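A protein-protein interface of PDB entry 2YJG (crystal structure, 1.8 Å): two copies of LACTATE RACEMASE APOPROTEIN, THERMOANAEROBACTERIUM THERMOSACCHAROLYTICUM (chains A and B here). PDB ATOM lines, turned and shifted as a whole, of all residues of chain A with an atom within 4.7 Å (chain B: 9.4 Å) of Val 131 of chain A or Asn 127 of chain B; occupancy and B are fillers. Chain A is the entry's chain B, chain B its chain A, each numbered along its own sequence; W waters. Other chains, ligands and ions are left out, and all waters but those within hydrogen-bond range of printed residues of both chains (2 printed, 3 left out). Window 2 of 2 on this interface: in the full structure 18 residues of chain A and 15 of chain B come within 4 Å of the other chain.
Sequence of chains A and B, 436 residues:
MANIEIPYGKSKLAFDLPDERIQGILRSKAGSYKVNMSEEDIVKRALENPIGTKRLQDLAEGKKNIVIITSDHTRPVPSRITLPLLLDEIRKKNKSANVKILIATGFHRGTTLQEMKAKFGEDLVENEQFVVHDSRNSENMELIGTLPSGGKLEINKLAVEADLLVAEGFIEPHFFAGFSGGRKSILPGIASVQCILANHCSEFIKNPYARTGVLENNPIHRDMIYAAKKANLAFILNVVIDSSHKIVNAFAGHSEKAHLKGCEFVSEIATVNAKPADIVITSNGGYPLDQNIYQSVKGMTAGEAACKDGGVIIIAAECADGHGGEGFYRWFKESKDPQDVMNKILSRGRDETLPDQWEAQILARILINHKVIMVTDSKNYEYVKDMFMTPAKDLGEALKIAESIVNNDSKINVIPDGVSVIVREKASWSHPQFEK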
ATOM      1  N   ILE A 101       5.018  19.824  33.031  1.00  0.00           N
ATOM      2  CA  ILE A 101       4.039  20.870  33.293  1.00  0.00           C
ATOM      3  C   ILE A 101       2.703  20.264  33.001  1.00  0.00           C
ATOM      4  O   ILE A 101       2.426  19.896  31.875  1.00  0.00           O
ATOM      5  CB  ILE A 101       4.320  22.122  32.433  1.00  0.00           C
ATOM      6  CG1 ILE A 101       5.738  22.638  32.725  1.00  0.00           C
ATOM      7  CG2 ILE A 101       3.205  23.201  32.581  1.00  0.00           C
ATOM      8  CD1 ILE A 101       6.409  23.178  31.468  1.00  0.00           C
ATOM      9  N   LEU A 102       1.909  20.119  34.055  1.00  0.00           N
ATOM     10  CA  LEU A 102       0.629  19.495  34.010  1.00  0.00           C
ATOM     11  C   LEU A 102      -0.509  20.547  33.945  1.00  0.00           C
ATOM     12  O   LEU A 102      -0.728  21.285  34.897  1.00  0.00           O
ATOM     13  CB  LEU A 102       0.492  18.567  35.234  1.00  0.00           C
ATOM     14  CG  LEU A 102      -0.860  17.837  35.322  1.00  0.00           C
ATOM     15  CD1 LEU A 102      -1.205  16.855  34.144  1.00  0.00           C
ATOM     16  CD2 LEU A 102      -0.863  17.058  36.592  1.00  0.00           C
ATOM     17  N   ILE A 103      -1.263  20.585  32.840  1.00  0.00           N
ATOM     18  CA  ILE A 103      -2.305  21.635  32.664  1.00  0.00           C
ATOM     19  C   ILE A 103      -3.586  21.236  33.408  1.00  0.00           C
ATOM     20  O   ILE A 103      -4.181  20.157  33.142  1.00  0.00           O
ATOM     21  CB  ILE A 103      -2.635  21.913  31.165  1.00  0.00           C
ATOM     22  CG1 ILE A 103      -1.390  22.235  30.327  1.00  0.00           C
ATOM     23  CG2 ILE A 103      -3.676  23.028  31.048  1.00  0.00           C
ATOM     24  CD1 ILE A 103      -0.635  23.305  30.811  1.00  0.00           C
ATOM     25  N   GLN A 129       8.090  19.575  28.521  1.00  0.00           N
ATOM     26  CA  GLN A 129       7.164  18.504  28.582  1.00  0.00           C
ATOM     27  C   GLN A 129       5.854  19.035  29.186  1.00  0.00           C
ATOM     28  O   GLN A 129       5.798  19.311  30.390  1.00  0.00           O
ATOM     29  CB  GLN A 129       7.695  17.375  29.513  1.00  0.00           C
ATOM     30  CG  GLN A 129       9.010  16.747  29.070  1.00  0.00           C
ATOM     31  CD  GLN A 129       9.616  15.903  30.119  1.00  0.00           C
ATOM     32  OE1 GLN A 129      10.534  16.365  30.873  1.00  0.00           O
ATOM     33  NE2 GLN A 129       9.099  14.697  30.261  1.00  0.00           N
ATOM     34  N   PHE A 130       4.845  19.177  28.358  1.00  0.00           N
ATOM     35  CA  PHE A 130       3.487  19.640  28.741  1.00  0.00           C
ATOM     36  C   PHE A 130       2.536  18.470  28.603  1.00  0.00           C
ATOM     37  O   PHE A 130       2.529  17.781  27.578  1.00  0.00           O
ATOM     38  CB  PHE A 130       2.994  20.748  27.820  1.00  0.00           C
ATOM     39  CG  PHE A 130       3.467  22.097  28.182  1.00  0.00           C
ATOM     40  CD1 PHE A 130       4.709  22.574  27.707  1.00  0.00           C
ATOM     41  CD2 PHE A 130       2.661  22.964  28.922  1.00  0.00           C
ATOM     42  CE1 PHE A 130       5.164  23.876  28.015  1.00  0.00           C
ATOM     43  CE2 PHE A 130       3.152  24.260  29.234  1.00  0.00           C
ATOM     44  CZ  PHE A 130       4.373  24.703  28.779  1.00  0.00           C
ATOM     45  N   VAL A 131       1.739  18.255  29.632  1.00  0.00           N
ATOM     46  CA  VAL A 131       0.809  17.149  29.720  1.00  0.00           C
ATOM     47  C   VAL A 131      -0.537  17.752  30.102  1.00  0.00           C
ATOM     48  O   VAL A 131      -0.621  18.599  31.020  1.00  0.00           O
ATOM     49  CB  VAL A 131       1.278  16.100  30.720  1.00  0.00           C
ATOM     50  CG1 VAL A 131       0.266  14.997  30.844  1.00  0.00           C
ATOM     51  CG2 VAL A 131       2.679  15.502  30.318  1.00  0.00           C
ATOM     52  N   VAL A 132      -1.600  17.329  29.411  1.00  0.00           N
ATOM     53  CA  VAL A 132      -2.938  17.849  29.685  1.00  0.00           C
ATOM     54  C   VAL A 132      -3.720  16.906  30.580  1.00  0.00           C
ATOM     55  O   VAL A 132      -3.876  15.781  30.259  1.00  0.00           O
ATOM     56  CB  VAL A 132      -3.713  18.095  28.361  1.00  0.00           C
ATOM     57  CG1 VAL A 132      -5.094  18.739  28.647  1.00  0.00           C
ATOM     58  CG2 VAL A 132      -2.862  19.006  27.359  1.00  0.00           C
ATOM     59  N   HIS A 133      -4.216  17.369  31.737  1.00  0.00           N
ATOM     60  CA  HIS A 133      -5.000  16.551  32.582  1.00  0.00           C
ATOM     61  C   HIS A 133      -6.311  16.164  31.905  1.00  0.00           C
ATOM     62  O   HIS A 133      -6.920  16.970  31.210  1.00  0.00           O
ATOM     63  CB  HIS A 133      -5.195  17.247  33.939  1.00  0.00           C
ATOM     64  CG  HIS A 133      -6.208  16.603  34.826  1.00  0.00           C
ATOM     65  ND1 HIS A 133      -5.986  15.427  35.521  1.00  0.00           N
ATOM     66  CD2 HIS A 133      -7.470  17.000  35.149  1.00  0.00           C
ATOM     67  CE1 HIS A 133      -7.077  15.131  36.210  1.00  0.00           C
ATOM     68  NE2 HIS A 133      -7.985  16.060  35.993  1.00  0.00           N
ATOM     69  N   LEU A 158       0.380  11.487  37.636  1.00  0.00           N
ATOM     70  CA  LEU A 158       1.641  12.167  37.417  1.00  0.00           C
ATOM     71  C   LEU A 158       1.974  13.034  38.622  1.00  0.00           C
ATOM     72  O   LEU A 158       3.129  13.140  39.027  1.00  0.00           O
ATOM     73  CB  LEU A 158       1.587  13.042  36.170  1.00  0.00           C
ATOM     74  CG  LEU A 158       2.910  13.601  35.729  1.00  0.00           C
ATOM     75  CD1 LEU A 158       3.849  12.444  35.328  1.00  0.00           C
ATOM     76  CD2 LEU A 158       2.734  14.561  34.568  1.00  0.00           C
ATOM     77  N   LEU B  87      11.483   5.902  22.528  1.00  0.00           N
ATOM     78  CA  LEU B  87      11.327   6.476  23.878  1.00  0.00           C
ATOM     79  C   LEU B  87      10.998   5.403  24.909  1.00  0.00           C
ATOM     80  O   LEU B  87      11.488   5.437  26.026  1.00  0.00           O
ATOM     81  CB  LEU B  87      10.221   7.527  23.851  1.00  0.00           C
ATOM     82  CG  LEU B  87      10.519   8.777  23.028  1.00  0.00           C
ATOM     83  CD1 LEU B  87       9.230   9.548  22.649  1.00  0.00           C
ATOM     84  CD2 LEU B  87      11.499   9.662  23.751  1.00  0.00           C
ATOM     85  N   ARG B  91      13.399   4.117  28.046  1.00  0.00           N
ATOM     86  CA  ARG B  91      12.853   4.244  29.415  1.00  0.00           C
ATOM     87  C   ARG B  91      12.799   2.905  30.134  1.00  0.00           C
ATOM     88  O   ARG B  91      12.613   2.863  31.365  1.00  0.00           O
ATOM     89  CB  ARG B  91      11.487   4.924  29.394  1.00  0.00           C
ATOM     90  CG  ARG B  91      11.637   6.431  29.073  1.00  0.00           C
ATOM     91  CD  ARG B  91      10.275   7.163  28.874  1.00  0.00           C
ATOM     92  NE  ARG B  91      10.493   8.597  28.806  1.00  0.00           N
ATOM     93  CZ  ARG B  91       9.896   9.460  28.000  1.00  0.00           C
ATOM     94  NH1 ARG B  91       9.008   9.087  27.079  1.00  0.00           N
ATOM     95  NH2 ARG B  91      10.226  10.741  28.092  1.00  0.00           N
ATOM     96  N   ALA B  97      14.614   9.147  32.537  1.00  0.00           N
ATOM     97  CA  ALA B  97      15.526   9.745  31.570  1.00  0.00           C
ATOM     98  C   ALA B  97      15.021  11.051  31.018  1.00  0.00           C
ATOM     99  O   ALA B  97      13.844  11.205  30.687  1.00  0.00           O
ATOM    100  CB  ALA B  97      15.811   8.781  30.392  1.00  0.00           C
ATOM    101  N   VAL B  99      15.042  13.121  27.891  1.00  0.00           N
ATOM    102  CA  VAL B  99      15.188  12.811  26.471  1.00  0.00           C
ATOM    103  C   VAL B  99      14.759  14.012  25.656  1.00  0.00           C
ATOM    104  O   VAL B  99      13.599  14.397  25.708  1.00  0.00           O
ATOM    105  CB  VAL B  99      14.384  11.610  26.033  1.00  0.00           C
ATOM    106  CG1 VAL B  99      14.697  11.241  24.510  1.00  0.00           C
ATOM    107  CG2 VAL B  99      14.685  10.460  26.850  1.00  0.00           C
ATOM    108  N   ILE B 101      14.416  15.637  21.786  1.00  0.00           N
ATOM    109  CA  ILE B 101      14.292  15.199  20.416  1.00  0.00           C
ATOM    110  C   ILE B 101      14.706  16.394  19.593  1.00  0.00           C
ATOM    111  O   ILE B 101      14.029  17.399  19.588  1.00  0.00           O
ATOM    112  CB  ILE B 101      12.857  14.688  20.135  1.00  0.00           C
ATOM    113  CG1 ILE B 101      12.546  13.498  21.060  1.00  0.00           C
ATOM    114  CG2 ILE B 101      12.707  14.203  18.733  1.00  0.00           C
ATOM    115  CD1 ILE B 101      11.075  13.145  21.153  1.00  0.00           C
ATOM    116  N   PHE B 120       4.502  14.589  13.909  1.00  0.00           N
ATOM    117  CA  PHE B 120       4.643  13.858  15.153  1.00  0.00           C
ATOM    118  C   PHE B 120       3.353  13.662  15.952  1.00  0.00           C
ATOM    119  O   PHE B 120       3.270  12.749  16.739  1.00  0.00           O
ATOM    120  CB  PHE B 120       5.696  14.573  16.032  1.00  0.00           C
ATOM    121  CG  PHE B 120       6.999  14.758  15.351  1.00  0.00           C
ATOM    122  CD1 PHE B 120       7.840  13.671  15.126  1.00  0.00           C
ATOM    123  CD2 PHE B 120       7.416  16.004  14.915  1.00  0.00           C
ATOM    124  CE1 PHE B 120       9.052  13.840  14.488  1.00  0.00           C
ATOM    125  CE2 PHE B 120       8.622  16.157  14.238  1.00  0.00           C
ATOM    126  CZ  PHE B 120       9.448  15.062  14.049  1.00  0.00           C
ATOM    127  N   GLY B 121       2.320  14.469  15.690  1.00  0.00           N
ATOM    128  CA  GLY B 121       1.088  14.382  16.455  1.00  0.00           C
ATOM    129  C   GLY B 121       1.172  15.316  17.659  1.00  0.00           C
ATOM    130  O   GLY B 121       2.244  15.566  18.210  1.00  0.00           O
ATOM    131  N   GLU B 122       0.012  15.821  18.059  1.00  0.00           N
ATOM    132  CA  GLU B 122      -0.122  16.824  19.078  1.00  0.00           C
ATOM    133  C   GLU B 122       0.412  16.389  20.457  1.00  0.00           C
ATOM    134  O   GLU B 122       1.139  17.132  21.105  1.00  0.00           O
ATOM    135  CB  GLU B 122      -1.612  17.123  19.129  1.00  0.00           C
ATOM    136  CG  GLU B 122      -2.085  18.094  20.075  1.00  0.00           C
ATOM    137  CD  GLU B 122      -3.360  18.760  19.562  1.00  0.00           C
ATOM    138  OE1 GLU B 122      -3.526  18.860  18.332  1.00  0.00           O
ATOM    139  OE2 GLU B 122      -4.150  19.211  20.395  1.00  0.00           O
ATOM    140  N   ASP B 123       0.077  15.182  20.871  1.00  0.00           N
ATOM    141  CA  ASP B 123       0.450  14.723  22.203  1.00  0.00           C
ATOM    142  C   ASP B 123       1.959  14.586  22.289  1.00  0.00           C
ATOM    143  O   ASP B 123       2.581  15.048  23.249  1.00  0.00           O
ATOM    144  CB  ASP B 123      -0.217  13.370  22.528  1.00  0.00           C
ATOM    145  CG  ASP B 123      -1.733  13.457  22.710  1.00  0.00           C
ATOM    146  OD1 ASP B 123      -2.324  14.544  22.799  1.00  0.00           O
ATOM    147  OD2 ASP B 123      -2.330  12.377  22.814  1.00  0.00           O
ATOM    148  N   LEU B 124       2.585  13.981  21.266  1.00  0.00           N
ATOM    149  CA  LEU B 124       4.020  13.795  21.302  1.00  0.00           C
ATOM    150  C   LEU B 124       4.782  15.153  21.319  1.00  0.00           C
ATOM    151  O   LEU B 124       5.741  15.338  22.096  1.00  0.00           O
ATOM    152  CB  LEU B 124       4.416  12.903  20.106  1.00  0.00           C
ATOM    153  CG  LEU B 124       5.680  12.085  20.036  1.00  0.00           C
ATOM    154  CD1 LEU B 124       5.871  11.291  21.322  1.00  0.00           C
ATOM    155  CD2 LEU B 124       5.573  11.150  18.762  1.00  0.00           C
ATOM    156  N   VAL B 125       4.312  16.131  20.533  1.00  0.00           N
ATOM    157  CA  VAL B 125       4.939  17.443  20.493  1.00  0.00           C
ATOM    158  C   VAL B 125       4.829  18.118  21.872  1.00  0.00           C
ATOM    159  O   VAL B 125       5.794  18.608  22.396  1.00  0.00           O
ATOM    160  CB  VAL B 125       4.367  18.336  19.351  1.00  0.00           C
ATOM    161  CG1 VAL B 125       4.800  19.770  19.479  1.00  0.00           C
ATOM    162  CG2 VAL B 125       4.757  17.770  17.950  1.00  0.00           C
ATOM    163  N   GLU B 126       3.655  18.075  22.463  1.00  0.00           N
ATOM    164  CA  GLU B 126       3.460  18.586  23.802  1.00  0.00           C
ATOM    165  C   GLU B 126       4.289  17.834  24.849  1.00  0.00           C
ATOM    166  O   GLU B 126       5.066  18.457  25.604  1.00  0.00           O
ATOM    167  CB  GLU B 126       1.968  18.506  24.159  1.00  0.00           C
ATOM    168  CG  GLU B 126       1.067  19.413  23.257  1.00  0.00           C
ATOM    169  CD  GLU B 126      -0.418  19.204  23.444  1.00  0.00           C
ATOM    170  OE1 GLU B 126      -0.835  18.321  24.247  1.00  0.00           O
ATOM    171  OE2 GLU B 126      -1.212  19.968  22.811  1.00  0.00           O
ATOM    172  N   ASN B 127       4.067  16.529  24.937  1.00  0.00           N
ATOM    173  CA  ASN B 127       4.468  15.709  26.057  1.00  0.00           C
ATOM    174  C   ASN B 127       6.006  15.500  26.144  1.00  0.00           C
ATOM    175  O   ASN B 127       6.564  15.227  27.227  1.00  0.00           O
ATOM    176  CB  ASN B 127       3.857  14.312  26.016  1.00  0.00           C
ATOM    177  CG  ASN B 127       2.335  14.236  26.248  1.00  0.00           C
ATOM    178  OD1 ASN B 127       1.607  15.199  26.609  1.00  0.00           O
ATOM    179  ND2 ASN B 127       1.840  13.073  25.970  1.00  0.00           N
ATOM    180  N   GLU B 128       6.682  15.531  24.998  1.00  0.00           N
ATOM    181  CA  GLU B 128       8.122  15.390  24.953  1.00  0.00           C
ATOM    182  C   GLU B 128       8.799  16.714  24.628  1.00  0.00           C
ATOM    183  O   GLU B 128       8.149  17.669  24.191  1.00  0.00           O
ATOM    184  CB  GLU B 128       8.542  14.336  23.932  1.00  0.00           C
ATOM    185  CG  GLU B 128       7.959  12.950  24.254  1.00  0.00           C
ATOM    186  CD  GLU B 128       8.401  12.276  25.513  1.00  0.00           C
ATOM    187  OE1 GLU B 128       9.402  12.655  26.133  1.00  0.00           O
ATOM    188  OE2 GLU B 128       7.688  11.320  25.924  1.00  0.00           O
ATOM    189  N   GLN B 129      10.114  16.728  24.815  1.00  0.00           N
ATOM    190  CA  GLN B 129      10.984  17.874  24.552  1.00  0.00           C
ATOM    191  C   GLN B 129      11.567  17.892  23.148  1.00  0.00           C
ATOM    192  O   GLN B 129      12.543  17.198  22.886  1.00  0.00           O
ATOM    193  CB  GLN B 129      12.162  17.888  25.551  1.00  0.00           C
ATOM    194  CG  GLN B 129      11.729  18.084  27.023  1.00  0.00           C
ATOM    195  CD  GLN B 129      12.892  18.252  27.950  1.00  0.00           C
ATOM    196  OE1 GLN B 129      13.516  17.273  28.365  1.00  0.00           O
ATOM    197  NE2 GLN B 129      13.226  19.500  28.272  1.00  0.00           N
ATOM    198  N   PHE B 130      10.982  18.689  22.275  1.00  0.00           N
ATOM    199  CA  PHE B 130      11.428  18.868  20.915  1.00  0.00           C
ATOM    200  C   PHE B 130      12.191  20.172  20.807  1.00  0.00           C
ATOM    201  O   PHE B 130      11.766  21.166  21.346  1.00  0.00           O
ATOM    202  CB  PHE B 130      10.229  18.940  19.939  1.00  0.00           C
ATOM    203  CG  PHE B 130       9.681  17.606  19.581  1.00  0.00           C
ATOM    204  CD1 PHE B 130       8.716  16.991  20.386  1.00  0.00           C
ATOM    205  CD2 PHE B 130      10.114  16.948  18.436  1.00  0.00           C
ATOM    206  CE1 PHE B 130       8.229  15.721  20.062  1.00  0.00           C
ATOM    207  CE2 PHE B 130       9.632  15.701  18.111  1.00  0.00           C
ATOM    208  CZ  PHE B 130       8.679  15.084  18.909  1.00  0.00           C
HETATM  209  O   HOH W   1      -1.187  15.360  27.272  1.00  0.00           O
HETATM  210  O   HOH W   2       6.282  13.756  29.187  1.00  0.00           O
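The backbone NH (N) of Phe 130 of chain A sits close to the backbone carbonyl oxygen (O) of Glu 126 of chain B. The side-chain amide oxygen (OD1) of Asn 127 of chain B sits close to the backbone carbonyl oxygen (O) of Phe 130 of chain A (2.9 Å).
The backbone NH (N) of Ile 101 of chain B is in hydrogen-bond range of the backbone carbonyl oxygen (O) of Gln 129 of chain B (2.7 Å). The backbone carbonyl oxygen (O) of Asp 123 of chain B lies close to the side-chain amide nitrogen (ND2) of Asn 127 of chain B (3.4 Å). The backbone NH (N) of Ile 101 of chain A lies within hydrogen-bond range of the backbone carbonyl oxygen (O) of Gln 129 of chain A (2.8 Å). N of Val 131 of chain A sits at hydrogen-bond distance from O of Ile 101 of chain A. O of Val 131 of chain A sits at hydrogen-bond distance from N of Ile 103 of chain A, 2.8 Å away.
Among the printed residues, pairs that only touch across the chains: Gln 129 of chain A with Glu 126 of chain B, Gln 129 of chain A with Asn 127 of chain B, Gln 129 of chain A with Gln 129 of chain B, Val 131 of chain A with Asn 127 of chain B and Val 132 of chain A with Glu 126 of chain B.
Printed residues of chain B within 4 Å of Gln 129 of chain A: Glu 126 (3.6 Å), Asn 127 (3.3 Å) and Gln 129 (3.7 Å). Of chain B, only Asn 127 (3.8 Å) comes within 4 Å of Val 131 of chain A. Val 132 of chain A touches just one residue of chain B: Glu 126. Of the printed residues of chain A, Glu 126 of chain B touches Gln 129, Phe 130 and Val 132. Asn 127 of chain B touches three residues of chain A.
Of the 9 printed residues of chain A, 4 touch a printed residue of chain B. Printed residues of chain A that touch a printed residue of chain B: Gln 129, Phe 130, Val 131 and Val 132. Hydrophobic or aromatic side chains of chain A within 4 Å of the printed part of chain B: Phe 130, Val 131 and Val 132. Among the printed residues, no Asp or Glu carboxylate lies within 4 Å of a Lys or Arg side-chain nitrogen of the other chain.
Gln 129 of chain A touches its own counterpart, Gln 129 of chain B.
Water W2 bridges O of Asn 127 of chain B (2.5 Å) and NE2 of Gln 129 of chain A (3.2 Å). Water W1 bridges OD1 of Asn 127 of chain B (2.9 Å) and N of Val 132 of chain A (2.9 Å).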
